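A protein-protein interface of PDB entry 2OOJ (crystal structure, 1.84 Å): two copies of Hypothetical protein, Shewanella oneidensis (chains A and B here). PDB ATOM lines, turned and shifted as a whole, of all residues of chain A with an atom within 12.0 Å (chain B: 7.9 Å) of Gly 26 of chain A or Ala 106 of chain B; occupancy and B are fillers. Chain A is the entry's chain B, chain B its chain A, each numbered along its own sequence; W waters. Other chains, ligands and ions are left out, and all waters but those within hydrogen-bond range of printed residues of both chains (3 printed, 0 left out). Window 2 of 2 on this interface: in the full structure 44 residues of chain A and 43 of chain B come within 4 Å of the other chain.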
ATOM      1  N   ALA A  22      17.392 -14.166  12.436  1.00  0.00           N
ATOM      2  CA  ALA A  22      16.587 -15.152  11.745  1.00  0.00           C
ATOM      3  C   ALA A  22      16.393 -16.423  12.582  1.00  0.00           C
ATOM      4  O   ALA A  22      17.164 -16.710  13.504  1.00  0.00           O
ATOM      5  CB  ALA A  22      17.264 -15.513  10.430  1.00  0.00           C
ATOM      6  N   THR A  23      15.403 -17.198  12.174  1.00  0.00           N
ATOM      7  CA  THR A  23      15.065 -18.486  12.772  1.00  0.00           C
ATOM      8  C   THR A  23      15.268 -19.571  11.743  1.00  0.00           C
ATOM      9  O   THR A  23      14.798 -19.472  10.615  1.00  0.00           O
ATOM     10  CB  THR A  23      13.610 -18.504  13.187  1.00  0.00           C
ATOM     11  OG1 THR A  23      13.394 -17.404  14.072  1.00  0.00           O
ATOM     12  CG2 THR A  23      13.239 -19.832  13.901  1.00  0.00           C
ATOM     13  N   GLY A  24      15.989 -20.596  12.138  1.00  0.00           N
ATOM     14  CA  GLY A  24      16.190 -21.732  11.281  1.00  0.00           C
ATOM     15  C   GLY A  24      14.922 -22.549  11.185  1.00  0.00           C
ATOM     16  O   GLY A  24      14.126 -22.592  12.121  1.00  0.00           O
ATOM     17  N   VAL A  25      14.739 -23.181  10.035  1.00  0.00           N
ATOM     18  CA  VAL A  25      13.636 -24.084   9.822  1.00  0.00           C
ATOM     19  C   VAL A  25      14.186 -25.319   9.150  1.00  0.00           C
ATOM     20  O   VAL A  25      15.351 -25.357   8.731  1.00  0.00           O
ATOM     21  CB  VAL A  25      12.485 -23.413   9.029  1.00  0.00           C
ATOM     22  CG1 VAL A  25      11.983 -22.181   9.775  1.00  0.00           C
ATOM     23  CG2 VAL A  25      12.904 -22.981   7.653  1.00  0.00           C
ATOM     24  N   GLY A  26      13.382 -26.369   9.121  1.00  0.00           N
ATOM     25  CA  GLY A  26      13.774 -27.582   8.429  1.00  0.00           C
ATOM     26  C   GLY A  26      14.933 -28.277   9.106  1.00  0.00           C
ATOM     27  O   GLY A  26      15.736 -28.951   8.449  1.00  0.00           O
ATOM     28  N   GLY A  27      15.016 -28.094  10.422  1.00  0.00           N
ATOM     29  CA  GLY A  27      16.042 -28.728  11.229  1.00  0.00           C
ATOM     30  C   GLY A  27      17.286 -27.886  11.387  1.00  0.00           C
ATOM     31  O   GLY A  27      18.168 -28.243  12.148  1.00  0.00           O
ATOM     32  N   VAL A  28      17.364 -26.757  10.680  1.00  0.00           N
ATOM     33  CA  VAL A  28      18.495 -25.843  10.858  1.00  0.00           C
ATOM     34  C   VAL A  28      18.398 -25.040  12.158  1.00  0.00           C
ATOM     35  O   VAL A  28      17.352 -24.547  12.507  1.00  0.00           O
ATOM     36  CB  VAL A  28      18.546 -24.880   9.658  1.00  0.00           C
ATOM     37  CG1 VAL A  28      19.518 -23.742   9.908  1.00  0.00           C
ATOM     38  CG2 VAL A  28      18.849 -25.673   8.368  1.00  0.00           C
ATOM     39  N   ASN A  29      19.503 -24.907  12.858  1.00  0.00           N
ATOM     40  CA  ASN A  29      19.631 -24.002  13.971  1.00  0.00           C
ATOM     41  C   ASN A  29      20.676 -22.910  13.654  1.00  0.00           C
ATOM     42  O   ASN A  29      21.840 -23.219  13.414  1.00  0.00           O
ATOM     43  CB  ASN A  29      20.046 -24.785  15.190  1.00  0.00           C
ATOM     44  CG  ASN A  29      18.904 -25.661  15.694  1.00  0.00           C
ATOM     45  OD1 ASN A  29      18.853 -26.844  15.404  1.00  0.00           O
ATOM     46  ND2 ASN A  29      17.929 -25.043  16.342  1.00  0.00           N
ATOM     47  N   LEU A  30      20.226 -21.663  13.727  1.00  0.00           N
ATOM     48  CA  LEU A  30      21.026 -20.503  13.352  1.00  0.00           C
ATOM     49  C   LEU A  30      21.520 -19.865  14.616  1.00  0.00           C
ATOM     50  O   LEU A  30      20.831 -19.871  15.650  1.00  0.00           O
ATOM     51  CB  LEU A  30      20.203 -19.481  12.575  1.00  0.00           C
ATOM     52  CG  LEU A  30      19.544 -19.925  11.285  1.00  0.00           C
ATOM     53  CD1 LEU A  30      18.805 -18.747  10.692  1.00  0.00           C
ATOM     54  CD2 LEU A  30      20.575 -20.517  10.291  1.00  0.00           C
ATOM     55  N   ALA A  54      25.117 -21.823  10.989  1.00  0.00           N
ATOM     56  CA  ALA A  54      23.958 -22.632  10.679  1.00  0.00           C
ATOM     57  C   ALA A  54      24.337 -24.097  10.879  1.00  0.00           C
ATOM     58  O   ALA A  54      25.155 -24.633  10.134  1.00  0.00           O
ATOM     59  CB  ALA A  54      23.533 -22.384   9.232  1.00  0.00           C
ATOM     60  N   MET A  55      23.797 -24.726  11.923  1.00  0.00           N
ATOM     61  CA  MET A  55      23.914 -26.164  12.124  1.00  0.00           C
ATOM     62  C   MET A  55      22.714 -26.822  11.441  1.00  0.00           C
ATOM     63  O   MET A  55      21.638 -26.308  11.505  1.00  0.00           O
ATOM     64  CB  MET A  55      23.888 -26.523  13.611  1.00  0.00           C
ATOM     65  CG  MET A  55      24.814 -25.705  14.491  1.00  0.00           C
ATOM     66  SD  MET A  55      26.708 -25.886  14.030  1.00  0.00           S
ATOM     67  CE  MET A  55      26.839 -27.871  14.130  1.00  0.00           C
ATOM     68  N   THR A  56      22.914 -27.929  10.752  1.00  0.00           N
ATOM     69  CA  THR A  56      21.816 -28.573  10.062  1.00  0.00           C
ATOM     70  C   THR A  56      21.359 -29.778  10.876  1.00  0.00           C
ATOM     71  O   THR A  56      21.939 -30.075  11.921  1.00  0.00           O
ATOM     72  CB  THR A  56      22.210 -28.990   8.668  1.00  0.00           C
ATOM     73  OG1 THR A  56      22.988 -30.177   8.737  1.00  0.00           O
ATOM     74  CG2 THR A  56      23.006 -27.835   7.931  1.00  0.00           C
ATOM     75  N   ALA A  57      20.344 -30.474  10.383  1.00  0.00           N
ATOM     76  CA  ALA A  57      19.854 -31.688  11.027  1.00  0.00           C
ATOM     77  C   ALA A  57      20.749 -32.893  10.779  1.00  0.00           C
ATOM     78  O   ALA A  57      20.521 -33.968  11.354  1.00  0.00           O
ATOM     79  CB  ALA A  57      18.419 -31.986  10.545  1.00  0.00           C
ATOM     80  N   VAL A  58      21.770 -32.752   9.934  1.00  0.00           N
ATOM     81  CA  VAL A  58      22.644 -33.871   9.625  1.00  0.00           C
ATOM     82  C   VAL A  58      23.957 -33.691  10.328  1.00  0.00           C
ATOM     83  O   VAL A  58      24.660 -32.703  10.119  1.00  0.00           O
ATOM     84  CB  VAL A  58      22.875 -33.993   8.126  1.00  0.00           C
ATOM     85  CG1 VAL A  58      23.949 -35.035   7.791  1.00  0.00           C
ATOM     86  CG2 VAL A  58      21.562 -34.314   7.442  1.00  0.00           C
ATOM     87  N   LYS A  59      24.283 -34.661  11.172  1.00  0.00           N
ATOM     88  CA  LYS A  59      25.531 -34.642  11.914  1.00  0.00           C
ATOM     89  C   LYS A  59      26.703 -34.391  10.996  1.00  0.00           C
ATOM     90  O   LYS A  59      26.872 -35.063   9.985  1.00  0.00           O
ATOM     91  CB  LYS A  59      25.750 -35.977  12.657  1.00  0.00           C
ATOM     92  CG  LYS A  59      24.990 -36.068  13.953  1.00  0.00           C
ATOM     93  CD  LYS A  59      25.553 -35.124  14.964  1.00  0.00           C
ATOM     94  CE  LYS A  59      24.944 -35.343  16.312  1.00  0.00           C
ATOM     95  NZ  LYS A  59      25.361 -34.223  17.218  1.00  0.00           N
ATOM     96  N   SER A  61      27.388 -31.624   9.369  1.00  0.00           N
ATOM     97  CA  SER A  61      27.116 -30.654   8.280  1.00  0.00           C
ATOM     98  C   SER A  61      26.666 -29.338   8.887  1.00  0.00           C
ATOM     99  O   SER A  61      25.665 -29.275   9.593  1.00  0.00           O
ATOM    100  CB  SER A  61      26.073 -31.191   7.284  1.00  0.00           C
ATOM    101  OG  SER A  61      26.645 -32.195   6.470  1.00  0.00           O
ATOM    102  N   ALA A  62      27.427 -28.272   8.621  1.00  0.00           N
ATOM    103  CA  ALA A  62      27.122 -26.978   9.171  1.00  0.00           C
ATOM    104  C   ALA A  62      27.939 -25.928   8.383  1.00  0.00           C
ATOM    105  O   ALA A  62      28.816 -26.275   7.596  1.00  0.00           O
ATOM    106  CB  ALA A  62      27.495 -26.929  10.625  1.00  0.00           C
ATOM    107  N   GLN B  69      18.543 -17.624   5.985  1.00  0.00           N
ATOM    108  CA  GLN B  69      17.587 -18.706   5.857  1.00  0.00           C
ATOM    109  C   GLN B  69      16.538 -18.336   4.830  1.00  0.00           C
ATOM    110  O   GLN B  69      15.791 -17.381   5.015  1.00  0.00           O
ATOM    111  CB  GLN B  69      16.916 -19.014   7.187  1.00  0.00           C
ATOM    112  CG  GLN B  69      15.807 -20.081   7.106  1.00  0.00           C
ATOM    113  CD  GLN B  69      16.320 -21.480   6.993  1.00  0.00           C
ATOM    114  OE1 GLN B  69      16.778 -22.070   7.978  1.00  0.00           O
ATOM    115  NE2 GLN B  69      16.174 -22.069   5.814  1.00  0.00           N
ATOM    116  N   VAL B  70      16.451 -19.148   3.788  1.00  0.00           N
ATOM    117  CA  VAL B  70      15.512 -18.972   2.698  1.00  0.00           C
ATOM    118  C   VAL B  70      14.356 -19.965   2.842  1.00  0.00           C
ATOM    119  O   VAL B  70      14.584 -21.138   3.187  1.00  0.00           O
ATOM    120  CB  VAL B  70      16.174 -19.203   1.344  1.00  0.00           C
ATOM    121  CG1 VAL B  70      15.177 -18.903   0.183  1.00  0.00           C
ATOM    122  CG2 VAL B  70      17.450 -18.375   1.220  1.00  0.00           C
ATOM    123  N   VAL B  71      13.127 -19.458   2.672  1.00  0.00           N
ATOM    124  CA  VAL B  71      11.914 -20.279   2.716  1.00  0.00           C
ATOM    125  C   VAL B  71      11.024 -19.945   1.526  1.00  0.00           C
ATOM    126  O   VAL B  71      10.673 -18.785   1.305  1.00  0.00           O
ATOM    127  CB  VAL B  71      11.128 -20.129   4.005  1.00  0.00           C
ATOM    128  CG1 VAL B  71       9.944 -21.101   4.003  1.00  0.00           C
ATOM    129  CG2 VAL B  71      12.030 -20.423   5.204  1.00  0.00           C
ATOM    130  N   GLY B  72      10.747 -20.951   0.706  1.00  0.00           N
ATOM    131  CA  GLY B  72       9.844 -20.779  -0.409  1.00  0.00           C
ATOM    132  C   GLY B  72       9.838 -21.939  -1.373  1.00  0.00           C
ATOM    133  O   GLY B  72       9.867 -23.082  -0.985  1.00  0.00           O
ATOM    134  N   ARG B  77       9.180 -26.588  -6.095  1.00  0.00           N
ATOM    135  CA  ARG B  77       9.399 -27.452  -4.941  1.00  0.00           C
ATOM    136  C   ARG B  77       9.450 -26.614  -3.708  1.00  0.00           C
ATOM    137  O   ARG B  77      10.246 -25.692  -3.615  1.00  0.00           O
ATOM    138  CB  ARG B  77      10.687 -28.219  -5.093  1.00  0.00           C
ATOM    139  CG  ARG B  77      10.747 -28.989  -6.378  1.00  0.00           C
ATOM    140  CD  ARG B  77      12.105 -29.614  -6.628  1.00  0.00           C
ATOM    141  NE  ARG B  77      12.410 -30.667  -5.663  1.00  0.00           N
ATOM    142  CZ  ARG B  77      13.319 -31.622  -5.847  1.00  0.00           C
ATOM    143  NH1 ARG B  77      14.011 -31.692  -6.974  1.00  0.00           N
ATOM    144  NH2 ARG B  77      13.534 -32.526  -4.901  1.00  0.00           N
ATOM    145  N   GLN B  78       8.608 -26.957  -2.742  1.00  0.00           N
ATOM    146  CA  GLN B  78       8.444 -26.145  -1.546  1.00  0.00           C
ATOM    147  C   GLN B  78       9.372 -26.611  -0.464  1.00  0.00           C
ATOM    148  O   GLN B  78       9.359 -27.785  -0.038  1.00  0.00           O
ATOM    149  CB  GLN B  78       6.991 -26.182  -1.061  1.00  0.00           C
ATOM    150  CG  GLN B  78       6.754 -25.504   0.282  1.00  0.00           C
ATOM    151  CD  GLN B  78       6.869 -23.976   0.238  1.00  0.00           C
ATOM    152  OE1 GLN B  78       6.328 -23.331  -0.664  1.00  0.00           O
ATOM    153  NE2 GLN B  78       7.541 -23.392   1.242  1.00  0.00           N
ATOM    154  N   GLY B  79      10.183 -25.686   0.023  1.00  0.00           N
ATOM    155  CA  GLY B  79      11.105 -26.052   1.070  1.00  0.00           C
ATOM    156  C   GLY B  79      11.886 -24.890   1.628  1.00  0.00           C
ATOM    157  O   GLY B  79      11.402 -23.760   1.685  1.00  0.00           O
ATOM    158  N   SER B  80      13.070 -25.198   2.116  1.00  0.00           N
ATOM    159  CA  SER B  80      13.942 -24.185   2.712  1.00  0.00           C
ATOM    160  C   SER B  80      15.397 -24.613   2.554  1.00  0.00           C
ATOM    161  O   SER B  80      15.680 -25.761   2.328  1.00  0.00           O
ATOM    162  CB  SER B  80      13.627 -24.002   4.187  1.00  0.00           C
ATOM    163  OG  SER B  80      13.841 -25.186   4.952  1.00  0.00           O
ATOM    164  N   PHE B  81      16.305 -23.636   2.628  1.00  0.00           N
ATOM    165  CA  PHE B  81      17.744 -23.896   2.587  1.00  0.00           C
ATOM    166  C   PHE B  81      18.447 -22.662   3.139  1.00  0.00           C
ATOM    167  O   PHE B  81      17.805 -21.622   3.323  1.00  0.00           O
ATOM    168  CB  PHE B  81      18.230 -24.263   1.190  1.00  0.00           C
ATOM    169  CG  PHE B  81      18.019 -23.189   0.146  1.00  0.00           C
ATOM    170  CD1 PHE B  81      16.810 -23.081  -0.514  1.00  0.00           C
ATOM    171  CD2 PHE B  81      19.036 -22.316  -0.176  1.00  0.00           C
ATOM    172  CE1 PHE B  81      16.606 -22.143  -1.486  1.00  0.00           C
ATOM    173  CE2 PHE B  81      18.852 -21.368  -1.161  1.00  0.00           C
ATOM    174  CZ  PHE B  81      17.616 -21.267  -1.808  1.00  0.00           C
ATOM    175  N   VAL B  82      19.732 -22.816   3.486  1.00  0.00           N
ATOM    176  CA  VAL B  82      20.553 -21.725   4.019  1.00  0.00           C
ATOM    177  C   VAL B  82      21.633 -21.344   2.990  1.00  0.00           C
ATOM    178  O   VAL B  82      22.303 -22.210   2.427  1.00  0.00           O
ATOM    179  CB  VAL B  82      21.231 -22.113   5.358  1.00  0.00           C
ATOM    180  CG1 VAL B  82      22.129 -20.981   5.926  1.00  0.00           C
ATOM    181  CG2 VAL B  82      20.158 -22.493   6.409  1.00  0.00           C
ATOM    182  N   HIS B 103      23.357 -29.937   3.371  1.00  0.00           N
ATOM    183  CA  HIS B 103      22.260 -30.542   4.155  1.00  0.00           C
ATOM    184  C   HIS B 103      21.359 -29.563   4.869  1.00  0.00           C
ATOM    185  O   HIS B 103      20.618 -29.951   5.766  1.00  0.00           O
ATOM    186  CB  HIS B 103      22.811 -31.558   5.138  1.00  0.00           C
ATOM    187  CG  HIS B 103      23.470 -32.689   4.446  1.00  0.00           C
ATOM    188  ND1 HIS B 103      24.823 -32.911   4.508  1.00  0.00           N
ATOM    189  CD2 HIS B 103      22.975 -33.601   3.577  1.00  0.00           C
ATOM    190  CE1 HIS B 103      25.135 -33.930   3.730  1.00  0.00           C
ATOM    191  NE2 HIS B 103      24.031 -34.373   3.161  1.00  0.00           N
ATOM    192  N   SER B 104      21.427 -28.296   4.469  1.00  0.00           N
ATOM    193  CA  SER B 104      20.488 -27.301   4.975  1.00  0.00           C
ATOM    194  C   SER B 104      19.127 -27.374   4.237  1.00  0.00           C
ATOM    195  O   SER B 104      18.128 -26.823   4.700  1.00  0.00           O
ATOM    196  CB  SER B 104      21.102 -25.907   4.886  1.00  0.00           C
ATOM    197  OG  SER B 104      21.153 -25.433   3.549  1.00  0.00           O
ATOM    198  N   GLY B 105      19.099 -28.051   3.089  1.00  0.00           N
ATOM    199  CA  GLY B 105      17.881 -28.149   2.279  1.00  0.00           C
ATOM    200  C   GLY B 105      16.864 -28.980   3.041  1.00  0.00           C
ATOM    201  O   GLY B 105      17.216 -29.977   3.637  1.00  0.00           O
ATOM    202  N   ALA B 106      15.617 -28.541   3.058  1.00  0.00           N
ATOM    203  CA  ALA B 106      14.571 -29.305   3.747  1.00  0.00           C
ATOM    204  C   ALA B 106      13.322 -29.324   2.900  1.00  0.00           C
ATOM    205  O   ALA B 106      13.209 -28.596   1.916  1.00  0.00           O
ATOM    206  CB  ALA B 106      14.285 -28.689   5.093  1.00  0.00           C
ATOM    207  N   GLY B 107      12.362 -30.172   3.270  1.00  0.00           N
ATOM    208  CA  GLY B 107      11.092 -30.160   2.582  1.00  0.00           C
ATOM    209  C   GLY B 107      11.341 -30.829   1.258  1.00  0.00           C
ATOM    210  O   GLY B 107      12.090 -31.788   1.195  1.00  0.00           O
ATOM    211  N   GLU B 108      10.764 -30.312   0.191  1.00  0.00           N
ATOM    212  CA  GLU B 108      11.054 -30.836  -1.142  1.00  0.00           C
ATOM    213  C   GLU B 108      12.387 -30.339  -1.687  1.00  0.00           C
ATOM    214  O   GLU B 108      12.732 -30.652  -2.828  1.00  0.00           O
ATOM    215  CB  GLU B 108       9.957 -30.444  -2.098  1.00  0.00           C
ATOM    216  CG  GLU B 108       8.585 -30.918  -1.657  1.00  0.00           C
ATOM    217  CD  GLU B 108       7.521 -30.589  -2.691  1.00  0.00           C
ATOM    218  OE1 GLU B 108       7.212 -29.391  -2.874  1.00  0.00           O
ATOM    219  OE2 GLU B 108       6.999 -31.540  -3.309  1.00  0.00           O
ATOM    220  N   LEU B 109      13.106 -29.532  -0.906  1.00  0.00           N
ATOM    221  CA  LEU B 109      14.443 -29.080  -1.295  1.00  0.00           C
ATOM    222  C   LEU B 109      15.546 -29.843  -0.580  1.00  0.00           C
ATOM    223  O   LEU B 109      16.722 -29.476  -0.646  1.00  0.00           O
ATOM    224  CB  LEU B 109      14.583 -27.587  -1.055  1.00  0.00           C
ATOM    225  CG  LEU B 109      13.594 -26.700  -1.804  1.00  0.00           C
ATOM    226  CD1 LEU B 109      13.898 -25.226  -1.576  1.00  0.00           C
ATOM    227  CD2 LEU B 109      13.626 -27.005  -3.259  1.00  0.00           C
ATOM    228  N   THR B 110      15.163 -30.904   0.129  1.00  0.00           N
ATOM    229  CA  THR B 110      16.124 -31.845   0.662  1.00  0.00           C
ATOM    230  C   THR B 110      17.089 -32.310  -0.403  1.00  0.00           C
ATOM    231  O   THR B 110      16.685 -32.665  -1.513  1.00  0.00           O
ATOM    232  CB  THR B 110      15.417 -33.089   1.280  1.00  0.00           C
ATOM    233  OG1 THR B 110      14.565 -32.653   2.340  1.00  0.00           O
ATOM    234  CG2 THR B 110      16.445 -34.066   1.849  1.00  0.00           C
ATOM    235  N   GLY B 111      18.372 -32.310  -0.077  1.00  0.00           N
ATOM    236  CA  GLY B 111      19.402 -32.731  -1.018  1.00  0.00           C
ATOM    237  C   GLY B 111      19.954 -31.581  -1.839  1.00  0.00           C
ATOM    238  O   GLY B 111      20.879 -31.766  -2.606  1.00  0.00           O
ATOM    239  N   LEU B 112      19.421 -30.368  -1.680  1.00  0.00           N
ATOM    240  CA  LEU B 112      19.913 -29.236  -2.499  1.00  0.00           C
ATOM    241  C   LEU B 112      21.405 -28.886  -2.298  1.00  0.00           C
ATOM    242  O   LEU B 112      21.907 -28.849  -1.166  1.00  0.00           O
ATOM    243  CB  LEU B 112      19.075 -27.965  -2.206  1.00  0.00           C
ATOM    244  CG  LEU B 112      19.306 -26.697  -3.031  1.00  0.00           C
ATOM    245  CD1 LEU B 112      18.890 -26.879  -4.489  1.00  0.00           C
ATOM    246  CD2 LEU B 112      18.503 -25.598  -2.394  1.00  0.00           C
ATOM    247  N   PHE B 133      20.414 -31.612  -6.988  1.00  0.00           N
ATOM    248  CA  PHE B 133      19.979 -32.361  -5.801  1.00  0.00           C
ATOM    249  C   PHE B 133      20.812 -33.630  -5.660  1.00  0.00           C
ATOM    250  O   PHE B 133      21.003 -34.330  -6.635  1.00  0.00           O
ATOM    251  CB  PHE B 133      18.481 -32.690  -5.882  1.00  0.00           C
ATOM    252  CG  PHE B 133      17.605 -31.476  -5.806  1.00  0.00           C
ATOM    253  CD1 PHE B 133      17.267 -30.941  -4.581  1.00  0.00           C
ATOM    254  CD2 PHE B 133      17.170 -30.845  -6.961  1.00  0.00           C
ATOM    255  CE1 PHE B 133      16.503 -29.800  -4.505  1.00  0.00           C
ATOM    256  CE2 PHE B 133      16.397 -29.725  -6.904  1.00  0.00           C
ATOM    257  CZ  PHE B 133      16.067 -29.175  -5.663  1.00  0.00           C
HETATM  258  O   HOH W   1      18.793 -29.361   8.141  1.00  0.00           O
HETATM  259  O   HOH W   2      16.371 -25.119   5.789  1.00  0.00           O
HETATM  260  O   HOH W   3      16.396 -31.317   6.091  1.00  0.00           O
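The side-chain amide nitrogen of Gln 69 of chain B lies within hydrogen-bond range of the backbone carbonyl oxygen of Phe 81 of chain B (3.0 Å).
The backbone NH (N) of Ala 106 of chain B is in hydrogen-bond range of the backbone carbonyl oxygen (O) of Ser 80 of chain B, at 2.9 Å.
N of Val 82 of chain B sits at hydrogen-bond distance from OG of Ser 104 of chain B, 3.0 Å away.
The side-chain hydroxyl (OG1) of Thr 56 of chain A lies within hydrogen-bond range of the backbone NH (N) of Val 58 of chain A, 3.1 Å away.
The backbone carbonyl oxygen of Ser 61 of chain A sits at hydrogen-bond distance from the side-chain hydroxyl of Thr 56 of chain A (3.0 Å).
Of chain B, only Ala 106 comes within 4 Å of Gly 26 of chain A.
Ala 106 of chain B touches just one residue of chain A: Gly 26 (3.6 Å).
Ser 80 of chain B touches one residue of chain A.
Of chain A, only Val 28 (3.9 Å) and Thr 56 (3.8 Å) come within 4 Å of Ser 104 of chain B.
No residue of chain A comes within 4 Å of Gly 105 of chain B.
No residue of chain A comes within 4 Å of Gly 107 of chain B.
Leu 109 of chain B touches none of the printed residues of chain A.
Of the printed residues of chain B, Val 28 of chain A touches Gln 69, Val 82 and Ser 104.
Printed residues of chain A within 4 Å of Val 71 of chain B: Val 25.
The nearest residue of chain B that does not touch Gly 26 of chain A is Ser 80 of chain B (4.2 Å).
The nearest printed residue of chain A that does not touch Val 71 of chain B is Thr 23 of chain A (6.2 Å).
Among the printed residues, no Asp or Glu carboxylate lies within 4 Å of a Lys or Arg side-chain nitrogen of the other chain.
The side-chain amide oxygen of Gln 69 of chain B lies within hydrogen-bond range of the backbone NH of Val 25 of chain A, at 3.1 Å.
The side-chain hydroxyl (OG) of Ser 61 of chain A sits at hydrogen-bond distance from a ring nitrogen (ND1) of His 103 of chain B (2.8 Å).
Gln 69 of chain B touches Gly 24 of chain A (OE1 to CA, 3.4 Å).
Val 71 of chain B touches Val 25 of chain A (CG2 to CG2, 3.6 Å).
Val 25 of chain A touches Ser 80 of chain B (CG2 to OG, 3.6 Å).
Gln 69 of chain B touches Val 28 of chain A (OE1 to CB, 3.7 Å).
Val 28 of chain A touches Val 82 of chain B (CG1 to CG2, 3.8 Å).
CG2 of Val 28 of chain A touches O of Ser 104 of chain B, 3.9 Å away.
Ala 54 of chain A touches Val 82 of chain B (CB to CG1, 3.9 Å).
His 103 of chain B touches Thr 56 of chain A.
N of Ser 104 of chain B touches CG2 of Thr 56 of chain A, 3.8 Å away.
Val 58 of chain A touches His 103 of chain B.
Water W2 lies within hydrogen-bond range of the side-chain hydroxyl of Ser 80 of chain B (2.7 Å), the backbone carbonyl oxygen of Ser 104 of chain B (2.7 Å), the side-chain amide nitrogen of Gln 69 of chain B (3.1 Å), the backbone carbonyl oxygen of Val 25 of chain A (3.1 Å) and the backbone NH of Phe 81 of chain B (3.5 Å).
Water W3 bridges O of Gly 105 of chain B (2.9 Å) and O of Gly 26 of chain A (3.4 Å).
Water W1 lies within hydrogen-bond range of N of Ala 57 of chain A, O of His 103 of chain B and O of Gly 26 of chain A.
No position is printed for both chains.
Of the 15 pairs that touch across the chains among the printed residues, none has its exchanged pair printed and touching as well.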
